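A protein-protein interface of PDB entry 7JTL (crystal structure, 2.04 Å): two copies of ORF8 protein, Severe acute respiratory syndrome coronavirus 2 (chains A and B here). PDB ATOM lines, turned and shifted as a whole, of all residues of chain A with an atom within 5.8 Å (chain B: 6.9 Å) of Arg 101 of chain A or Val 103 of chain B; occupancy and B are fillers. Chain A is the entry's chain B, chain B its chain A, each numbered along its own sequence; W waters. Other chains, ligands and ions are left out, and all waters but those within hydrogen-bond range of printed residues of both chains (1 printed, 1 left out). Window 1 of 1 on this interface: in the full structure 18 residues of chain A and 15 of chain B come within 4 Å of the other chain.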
ATOM      1  N   GLU A   5     -27.408  24.721  18.372  1.00  0.00           N
ATOM      2  CA  GLU A   5     -28.144  23.749  19.158  1.00  0.00           C
ATOM      3  C   GLU A   5     -29.006  22.855  18.280  1.00  0.00           C
ATOM      4  O   GLU A   5     -29.523  23.255  17.233  1.00  0.00           O
ATOM      5  CB  GLU A   5     -29.012  24.432  20.211  1.00  0.00           C
ATOM      6  CG  GLU A   5     -28.457  24.263  21.615  1.00  0.00           C
ATOM      7  CD  GLU A   5     -29.074  25.233  22.599  1.00  0.00           C
ATOM      8  OE1 GLU A   5     -30.204  25.708  22.313  1.00  0.00           O
ATOM      9  OE2 GLU A   5     -28.440  25.526  23.643  1.00  0.00           O
ATOM     10  N   CYS A   6     -29.168  21.638  18.748  1.00  0.00           N
ATOM     11  CA  CYS A   6     -29.915  20.618  18.049  1.00  0.00           C
ATOM     12  C   CYS A   6     -30.972  20.037  18.972  1.00  0.00           C
ATOM     13  O   CYS A   6     -30.746  19.887  20.177  1.00  0.00           O
ATOM     14  CB  CYS A   6     -28.993  19.515  17.563  1.00  0.00           C
ATOM     15  SG  CYS A   6     -29.907  18.311  16.647  1.00  0.00           S
ATOM     16  N   SER A   7     -32.135  19.738  18.402  1.00  0.00           N
ATOM     17  CA  SER A   7     -33.246  19.193  19.163  1.00  0.00           C
ATOM     18  C   SER A   7     -33.711  17.924  18.472  1.00  0.00           C
ATOM     19  O   SER A   7     -34.276  17.981  17.377  1.00  0.00           O
ATOM     20  CB  SER A   7     -34.382  20.200  19.286  1.00  0.00           C
ATOM     21  OG  SER A   7     -35.523  19.568  19.840  1.00  0.00           O
ATOM     22  N   LEU A   8     -33.448  16.789  19.102  1.00  0.00           N
ATOM     23  CA  LEU A   8     -33.836  15.486  18.587  1.00  0.00           C
ATOM     24  C   LEU A   8     -35.144  15.073  19.248  1.00  0.00           C
ATOM     25  O   LEU A   8     -35.230  15.008  20.477  1.00  0.00           O
ATOM     26  CB  LEU A   8     -32.751  14.442  18.842  1.00  0.00           C
ATOM     27  CG  LEU A   8     -33.103  13.013  18.430  1.00  0.00           C
ATOM     28  CD1 LEU A   8     -33.495  12.962  16.966  1.00  0.00           C
ATOM     29  CD2 LEU A   8     -31.901  12.106  18.686  1.00  0.00           C
ATOM     30  N   ALA A  37     -30.681  22.671   3.883  1.00  0.00           N
ATOM     31  CA  ALA A  37     -29.934  22.677   5.136  1.00  0.00           C
ATOM     32  C   ALA A  37     -28.606  23.413   4.984  1.00  0.00           C
ATOM     33  O   ALA A  37     -27.680  23.208   5.773  1.00  0.00           O
ATOM     34  CB  ALA A  37     -29.709  21.253   5.664  1.00  0.00           C
ATOM     35  N   SER A  83     -33.721  21.925   6.078  1.00  0.00           N
ATOM     36  CA  SER A  83     -33.827  21.561   7.481  1.00  0.00           C
ATOM     37  C   SER A  83     -34.931  22.346   8.183  1.00  0.00           C
ATOM     38  O   SER A  83     -35.279  23.472   7.798  1.00  0.00           O
ATOM     39  CB  SER A  83     -32.513  21.815   8.192  1.00  0.00           C
ATOM     40  OG  SER A  83     -32.147  23.148   7.981  1.00  0.00           O
ATOM     41  N   LEU A  84     -35.507  21.724   9.206  1.00  0.00           N
ATOM     42  CA  LEU A  84     -36.492  22.395  10.036  1.00  0.00           C
ATOM     43  C   LEU A  84     -35.762  23.158  11.127  1.00  0.00           C
ATOM     44  O   LEU A  84     -35.041  22.568  11.935  1.00  0.00           O
ATOM     45  CB  LEU A  84     -37.478  21.406  10.634  1.00  0.00           C
ATOM     46  CG  LEU A  84     -38.474  22.129  11.537  1.00  0.00           C
ATOM     47  CD1 LEU A  84     -39.301  23.144  10.742  1.00  0.00           C
ATOM     48  CD2 LEU A  84     -39.369  21.107  12.220  1.00  0.00           C
ATOM     49  N   VAL A  85     -35.936  24.459  11.150  1.00  0.00           N
ATOM     50  CA  VAL A  85     -35.216  25.303  12.089  1.00  0.00           C
ATOM     51  C   VAL A  85     -36.218  26.194  12.797  1.00  0.00           C
ATOM     52  O   VAL A  85     -37.125  26.731  12.159  1.00  0.00           O
ATOM     53  CB  VAL A  85     -34.142  26.144  11.368  1.00  0.00           C
ATOM     54  CG1 VAL A  85     -33.486  27.084  12.336  1.00  0.00           C
ATOM     55  CG2 VAL A  85     -33.094  25.210  10.763  1.00  0.00           C
ATOM     56  N   VAL A  86     -36.052  26.353  14.110  1.00  0.00           N
ATOM     57  CA  VAL A  86     -36.836  27.298  14.890  1.00  0.00           C
ATOM     58  C   VAL A  86     -35.910  28.428  15.314  1.00  0.00           C
ATOM     59  O   VAL A  86     -34.767  28.189  15.731  1.00  0.00           O
ATOM     60  CB  VAL A  86     -37.511  26.636  16.106  1.00  0.00           C
ATOM     61  CG1 VAL A  86     -36.479  26.122  17.093  1.00  0.00           C
ATOM     62  CG2 VAL A  86     -38.468  27.629  16.772  1.00  0.00           C
ATOM     63  N   ASP A  99     -30.948  30.065  16.773  1.00  0.00           N
ATOM     64  CA  ASP A  99     -31.631  29.063  15.972  1.00  0.00           C
ATOM     65  C   ASP A  99     -31.385  27.681  16.541  1.00  0.00           C
ATOM     66  O   ASP A  99     -30.285  27.383  17.006  1.00  0.00           O
ATOM     67  CB  ASP A  99     -31.150  29.083  14.524  1.00  0.00           C
ATOM     68  CG  ASP A  99     -31.550  30.328  13.804  1.00  0.00           C
ATOM     69  OD1 ASP A  99     -32.499  30.985  14.279  1.00  0.00           O
ATOM     70  OD2 ASP A  99     -30.944  30.627  12.748  1.00  0.00           O
ATOM     71  N   VAL A 100     -32.408  26.840  16.496  1.00  0.00           N
ATOM     72  CA  VAL A 100     -32.288  25.439  16.880  1.00  0.00           C
ATOM     73  C   VAL A 100     -32.809  24.599  15.728  1.00  0.00           C
ATOM     74  O   VAL A 100     -33.927  24.826  15.257  1.00  0.00           O
ATOM     75  CB  VAL A 100     -33.064  25.123  18.174  1.00  0.00           C
ATOM     76  CG1 VAL A 100     -32.822  23.677  18.590  1.00  0.00           C
ATOM     77  CG2 VAL A 100     -32.689  26.096  19.286  1.00  0.00           C
ATOM     78  N   ARG A 101     -32.004  23.649  15.258  1.00  0.00           N
ATOM     79  CA  ARG A 101     -32.482  22.698  14.266  1.00  0.00           C
ATOM     80  C   ARG A 101     -33.248  21.574  14.953  1.00  0.00           C
ATOM     81  O   ARG A 101     -32.868  21.109  16.033  1.00  0.00           O
ATOM     82  CB  ARG A 101     -31.324  22.122  13.451  1.00  0.00           C
ATOM     83  CG  ARG A 101     -31.793  21.170  12.373  1.00  0.00           C
ATOM     84  CD  ARG A 101     -30.706  20.898  11.373  1.00  0.00           C
ATOM     85  NE  ARG A 101     -31.038  19.804  10.470  1.00  0.00           N
ATOM     86  CZ  ARG A 101     -30.240  19.428   9.480  1.00  0.00           C
ATOM     87  NH1 ARG A 101     -29.084  20.058   9.305  1.00  0.00           N
ATOM     88  NH2 ARG A 101     -30.565  18.410   8.697  1.00  0.00           N
ATOM     89  N   VAL A 102     -34.342  21.139  14.336  1.00  0.00           N
ATOM     90  CA  VAL A 102     -35.155  20.058  14.880  1.00  0.00           C
ATOM     91  C   VAL A 102     -35.057  18.849  13.976  1.00  0.00           C
ATOM     92  O   VAL A 102     -35.318  18.947  12.774  1.00  0.00           O
ATOM     93  CB  VAL A 102     -36.612  20.499  15.049  1.00  0.00           C
ATOM     94  CG1 VAL A 102     -37.496  19.303  15.374  1.00  0.00           C
ATOM     95  CG2 VAL A 102     -36.669  21.521  16.149  1.00  0.00           C
ATOM     96  N   VAL A 103     -34.743  17.698  14.557  1.00  0.00           N
ATOM     97  CA  VAL A 103     -34.543  16.480  13.795  1.00  0.00           C
ATOM     98  C   VAL A 103     -35.358  15.358  14.430  1.00  0.00           C
ATOM     99  O   VAL A 103     -35.519  15.304  15.653  1.00  0.00           O
ATOM    100  CB  VAL A 103     -33.030  16.151  13.711  1.00  0.00           C
ATOM    101  CG1 VAL A 103     -32.412  16.125  15.091  1.00  0.00           C
ATOM    102  CG2 VAL A 103     -32.818  14.838  13.059  1.00  0.00           C
ATOM    103  N   CYS B   6     -27.883  14.794  20.332  1.00  0.00           N
ATOM    104  CA  CYS B   6     -27.699  15.262  18.964  1.00  0.00           C
ATOM    105  C   CYS B   6     -26.422  16.093  18.845  1.00  0.00           C
ATOM    106  O   CYS B   6     -26.077  16.861  19.749  1.00  0.00           O
ATOM    107  CB  CYS B   6     -28.909  16.080  18.511  1.00  0.00           C
ATOM    108  SG  CYS B   6     -28.783  16.592  16.793  1.00  0.00           S
ATOM    109  N   SER B   7     -25.719  15.922  17.731  1.00  0.00           N
ATOM    110  CA  SER B   7     -24.465  16.619  17.457  1.00  0.00           C
ATOM    111  C   SER B   7     -24.653  17.272  16.097  1.00  0.00           C
ATOM    112  O   SER B   7     -24.741  16.573  15.081  1.00  0.00           O
ATOM    113  CB  SER B   7     -23.274  15.651  17.468  1.00  0.00           C
ATOM    114  OG  SER B   7     -22.066  16.225  16.959  1.00  0.00           O
ATOM    115  N   LEU B   8     -24.761  18.599  16.082  1.00  0.00           N
ATOM    116  CA  LEU B   8     -24.983  19.355  14.855  1.00  0.00           C
ATOM    117  C   LEU B   8     -23.631  19.840  14.340  1.00  0.00           C
ATOM    118  O   LEU B   8     -22.917  20.554  15.047  1.00  0.00           O
ATOM    119  CB  LEU B   8     -25.915  20.538  15.104  1.00  0.00           C
ATOM    120  CG  LEU B   8     -26.145  21.445  13.897  1.00  0.00           C
ATOM    121  CD1 LEU B   8     -26.722  20.638  12.749  1.00  0.00           C
ATOM    122  CD2 LEU B   8     -27.032  22.610  14.243  1.00  0.00           C
ATOM    123  N   GLN B   9     -23.282  19.465  13.117  1.00  0.00           N
ATOM    124  CA  GLN B   9     -21.969  19.785  12.585  1.00  0.00           C
ATOM    125  C   GLN B   9     -22.127  20.403  11.213  1.00  0.00           C
ATOM    126  O   GLN B   9     -23.165  20.261  10.567  1.00  0.00           O
ATOM    127  CB  GLN B   9     -21.052  18.546  12.541  1.00  0.00           C
ATOM    128  CG  GLN B   9     -20.766  18.017  13.943  1.00  0.00           C
ATOM    129  CD  GLN B   9     -19.850  16.823  13.959  1.00  0.00           C
ATOM    130  OE1 GLN B   9     -18.979  16.680  13.102  1.00  0.00           O
ATOM    131  NE2 GLN B   9     -20.035  15.954  14.943  1.00  0.00           N
ATOM    132  N   SER B  10     -21.085  21.112  10.790  1.00  0.00           N
ATOM    133  CA  SER B  10     -21.076  21.870   9.543  1.00  0.00           C
ATOM    134  C   SER B  10     -19.929  21.407   8.661  1.00  0.00           C
ATOM    135  O   SER B  10     -18.813  21.214   9.140  1.00  0.00           O
ATOM    136  CB  SER B  10     -20.924  23.389   9.790  1.00  0.00           C
ATOM    137  OG  SER B  10     -21.967  23.895  10.598  1.00  0.00           O
ATOM    138  N   GLU B  78     -26.116  13.962   3.967  1.00  0.00           N
ATOM    139  CA  GLU B  78     -27.002  13.132   4.783  1.00  0.00           C
ATOM    140  C   GLU B  78     -27.176  11.793   4.067  1.00  0.00           C
ATOM    141  O   GLU B  78     -27.587  11.786   2.904  1.00  0.00           O
ATOM    142  CB  GLU B  78     -28.360  13.817   4.957  1.00  0.00           C
ATOM    143  CG  GLU B  78     -28.365  15.082   5.862  1.00  0.00           C
ATOM    144  CD  GLU B  78     -28.007  14.849   7.359  1.00  0.00           C
ATOM    145  OE1 GLU B  78     -27.822  13.676   7.770  1.00  0.00           O
ATOM    146  OE2 GLU B  78     -27.932  15.839   8.140  1.00  0.00           O
ATOM    147  N   LEU B  84     -27.062   9.044  10.731  1.00  0.00           N
ATOM    148  CA  LEU B  84     -25.714   8.746  11.182  1.00  0.00           C
ATOM    149  C   LEU B  84     -25.694   8.782  12.701  1.00  0.00           C
ATOM    150  O   LEU B  84     -26.065   9.786  13.306  1.00  0.00           O
ATOM    151  CB  LEU B  84     -24.716   9.750  10.611  1.00  0.00           C
ATOM    152  CG  LEU B  84     -23.280   9.478  11.041  1.00  0.00           C
ATOM    153  CD1 LEU B  84     -22.793   8.112  10.495  1.00  0.00           C
ATOM    154  CD2 LEU B  84     -22.368  10.608  10.607  1.00  0.00           C
ATOM    155  N   ARG B 101     -26.764  11.012  17.702  1.00  0.00           N
ATOM    156  CA  ARG B 101     -27.021  11.233  16.287  1.00  0.00           C
ATOM    157  C   ARG B 101     -26.230  12.435  15.783  1.00  0.00           C
ATOM    158  O   ARG B 101     -26.145  13.466  16.450  1.00  0.00           O
ATOM    159  CB  ARG B 101     -28.512  11.448  16.060  1.00  0.00           C
ATOM    160  CG  ARG B 101     -28.869  11.635  14.609  1.00  0.00           C
ATOM    161  CD  ARG B 101     -30.336  11.515  14.379  1.00  0.00           C
ATOM    162  NE  ARG B 101     -30.680  11.939  13.030  1.00  0.00           N
ATOM    163  CZ  ARG B 101     -31.902  11.875  12.521  1.00  0.00           C
ATOM    164  NH1 ARG B 101     -32.910  11.415  13.253  1.00  0.00           N
ATOM    165  NH2 ARG B 101     -32.117  12.284  11.279  1.00  0.00           N
ATOM    166  N   VAL B 102     -25.650  12.311  14.596  1.00  0.00           N
ATOM    167  CA  VAL B 102     -24.894  13.398  14.000  1.00  0.00           C
ATOM    168  C   VAL B 102     -25.681  13.922  12.817  1.00  0.00           C
ATOM    169  O   VAL B 102     -26.090  13.149  11.940  1.00  0.00           O
ATOM    170  CB  VAL B 102     -23.480  12.966  13.578  1.00  0.00           C
ATOM    171  CG1 VAL B 102     -22.831  14.066  12.751  1.00  0.00           C
ATOM    172  CG2 VAL B 102     -22.632  12.668  14.808  1.00  0.00           C
ATOM    173  N   VAL B 103     -25.854  15.244  12.780  1.00  0.00           N
ATOM    174  CA  VAL B 103     -26.637  15.955  11.786  1.00  0.00           C
ATOM    175  C   VAL B 103     -25.730  16.996  11.154  1.00  0.00           C
ATOM    176  O   VAL B 103     -24.889  17.583  11.844  1.00  0.00           O
ATOM    177  CB  VAL B 103     -27.841  16.643  12.457  1.00  0.00           C
ATOM    178  CG1 VAL B 103     -28.704  17.334  11.447  1.00  0.00           C
ATOM    179  CG2 VAL B 103     -28.615  15.653  13.280  1.00  0.00           C
ATOM    180  N   LEU B 104     -25.894  17.235   9.857  1.00  0.00           N
ATOM    181  CA  LEU B 104     -25.044  18.169   9.130  1.00  0.00           C
ATOM    182  C   LEU B 104     -25.825  19.405   8.711  1.00  0.00           C
ATOM    183  O   LEU B 104     -26.831  19.300   8.008  1.00  0.00           O
ATOM    184  CB  LEU B 104     -24.416  17.522   7.879  1.00  0.00           C
ATOM    185  CG  LEU B 104     -23.644  16.221   8.039  1.00  0.00           C
ATOM    186  CD1 LEU B 104     -23.012  15.794   6.710  1.00  0.00           C
ATOM    187  CD2 LEU B 104     -22.586  16.367   9.126  1.00  0.00           C
ATOM    188  N   ASP B 105     -25.322  20.572   9.092  1.00  0.00           N
ATOM    189  CA  ASP B 105     -25.585  21.792   8.348  1.00  0.00           C
ATOM    190  C   ASP B 105     -24.504  21.901   7.278  1.00  0.00           C
ATOM    191  O   ASP B 105     -23.346  21.559   7.523  1.00  0.00           O
ATOM    192  CB  ASP B 105     -25.550  23.022   9.261  1.00  0.00           C
ATOM    193  CG  ASP B 105     -26.822  23.183  10.095  1.00  0.00           C
ATOM    194  OD1 ASP B 105     -27.796  22.413   9.887  1.00  0.00           O
ATOM    195  OD2 ASP B 105     -26.837  24.086  10.958  1.00  0.00           O
ATOM    196  N   PHE B 106     -24.874  22.385   6.100  1.00  0.00           N
ATOM    197  CA  PHE B 106     -23.928  22.503   5.002  1.00  0.00           C
ATOM    198  C   PHE B 106     -23.469  23.941   4.869  1.00  0.00           C
ATOM    199  O   PHE B 106     -24.262  24.872   5.020  1.00  0.00           O
ATOM    200  CB  PHE B 106     -24.546  22.023   3.690  1.00  0.00           C
ATOM    201  CG  PHE B 106     -25.060  20.622   3.761  1.00  0.00           C
ATOM    202  CD1 PHE B 106     -24.174  19.558   3.921  1.00  0.00           C
ATOM    203  CD2 PHE B 106     -26.411  20.361   3.690  1.00  0.00           C
ATOM    204  CE1 PHE B 106     -24.639  18.265   3.996  1.00  0.00           C
ATOM    205  CE2 PHE B 106     -26.885  19.072   3.765  1.00  0.00           C
ATOM    206  CZ  PHE B 106     -26.006  18.024   3.916  1.00  0.00           C
HETATM  207  O   HOH W   1     -30.151  24.079   9.219  1.00  0.00           O
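OD1 of Asp 105 of chain B lies within salt-bridge range of NH1 of Arg 101 of chain A (2.7 Å).
The side-chain sulfur (SG) of Cys 6 of chain A forms a disulfide with the side-chain sulfur (SG) of Cys 6 of chain B, at 2.1 Å.
NH1 of Arg 101 of chain A lies within hydrogen-bond range of O of Leu 104 of chain B (2.7 Å).
The side-chain carboxylate (OE2) of Glu 78 of chain B is in salt-bridge range of the guanidinium group (NH2) of Arg 101 of chain A, at 3.7 Å.
O of Ala 37 of chain A lies within hydrogen-bond range of N of Phe 106 of chain B (2.9 Å).
The backbone carbonyl oxygen of Glu 5 of chain A sits at hydrogen-bond distance from the backbone NH of Arg 101 of chain A, at 3.2 Å.
O of Ser 7 of chain B lies within hydrogen-bond range of N of Val 103 of chain B, 2.9 Å away.
O of Arg 101 of chain A is in hydrogen-bond range of N of Ser 7 of chain A.
O of Ser 7 of chain A is in hydrogen-bond range of N of Val 103 of chain A (2.9 Å).
The backbone NH (N) of Asp 105 of chain B sits at hydrogen-bond distance from the backbone carbonyl oxygen (O) of Gln 9 of chain B (2.6 Å).
The backbone NH (N) of Leu 104 of chain B is in hydrogen-bond range of the side-chain carboxylate (OE2) of Glu 78 of chain B.
Among the printed residues, pairs that only touch across the chains: Glu 5 of chain A with Leu 8 of chain B, Ala 37 of chain A with Asp 105 of chain B, Arg 101 of chain A with Val 103 of chain B and Val 103 of chain A with Arg 101 of chain B.
Arg 101 of chain A touches just these residues of chain B: Glu 78 (3.7 Å), Val 103 (3.3 Å), Leu 104 (2.7 Å) and Asp 105 (2.7 Å).
Printed residues of chain A within 4 Å of Val 103 of chain B: Arg 101.
Printed residues of chain A within 4 Å of Phe 106 of chain B: Ala 37 (2.9 Å).
Of the printed residues of chain B, Ala 37 of chain A touches Asp 105 and Phe 106.
Printed residues of chain A within 4 Å of Leu 8 of chain B: Glu 5.
Of the printed residues of chain A, Arg 101 of chain B touches Val 103.
The nearest residue of chain B that does not touch Arg 101 of chain A is Leu 8 of chain B (4.2 Å).
The nearest printed residue of chain B that does not touch Ala 37 of chain A is Leu 104 of chain B (4.2 Å).
Printed residues of chain A that touch a printed residue of chain B: Glu 5, Cys 6, Ala 37, Arg 101 and Val 103.
Of the 13 printed residues of chain B, 8 touch a printed residue of chain A.
Printed residues of chain B that touch a printed residue of chain A: Cys 6, Leu 8, Glu 78, Arg 101, Val 103, Leu 104, Asp 105 and Phe 106.
Hydrophobic or aromatic side chains of chain B within 4 Å of the printed part of chain A: Leu 8, Val 103 and Phe 106.
Cys 6 of chain B touches its own counterpart, Cys 6 of chain A.
Arg 101 of chain A touches Val 103 of chain B, and with the chains exchanged Val 103 of chain A touches Arg 101 of chain B.
Of the 9 pairs that touch across the chains among the printed residues, 3 have their exchanged pair printed and touching as well.
Water W1 lies within hydrogen-bond range of OG of Ser 83 of chain A (2.5 Å) and OD1 of Asp 105 of chain B (3.0 Å).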
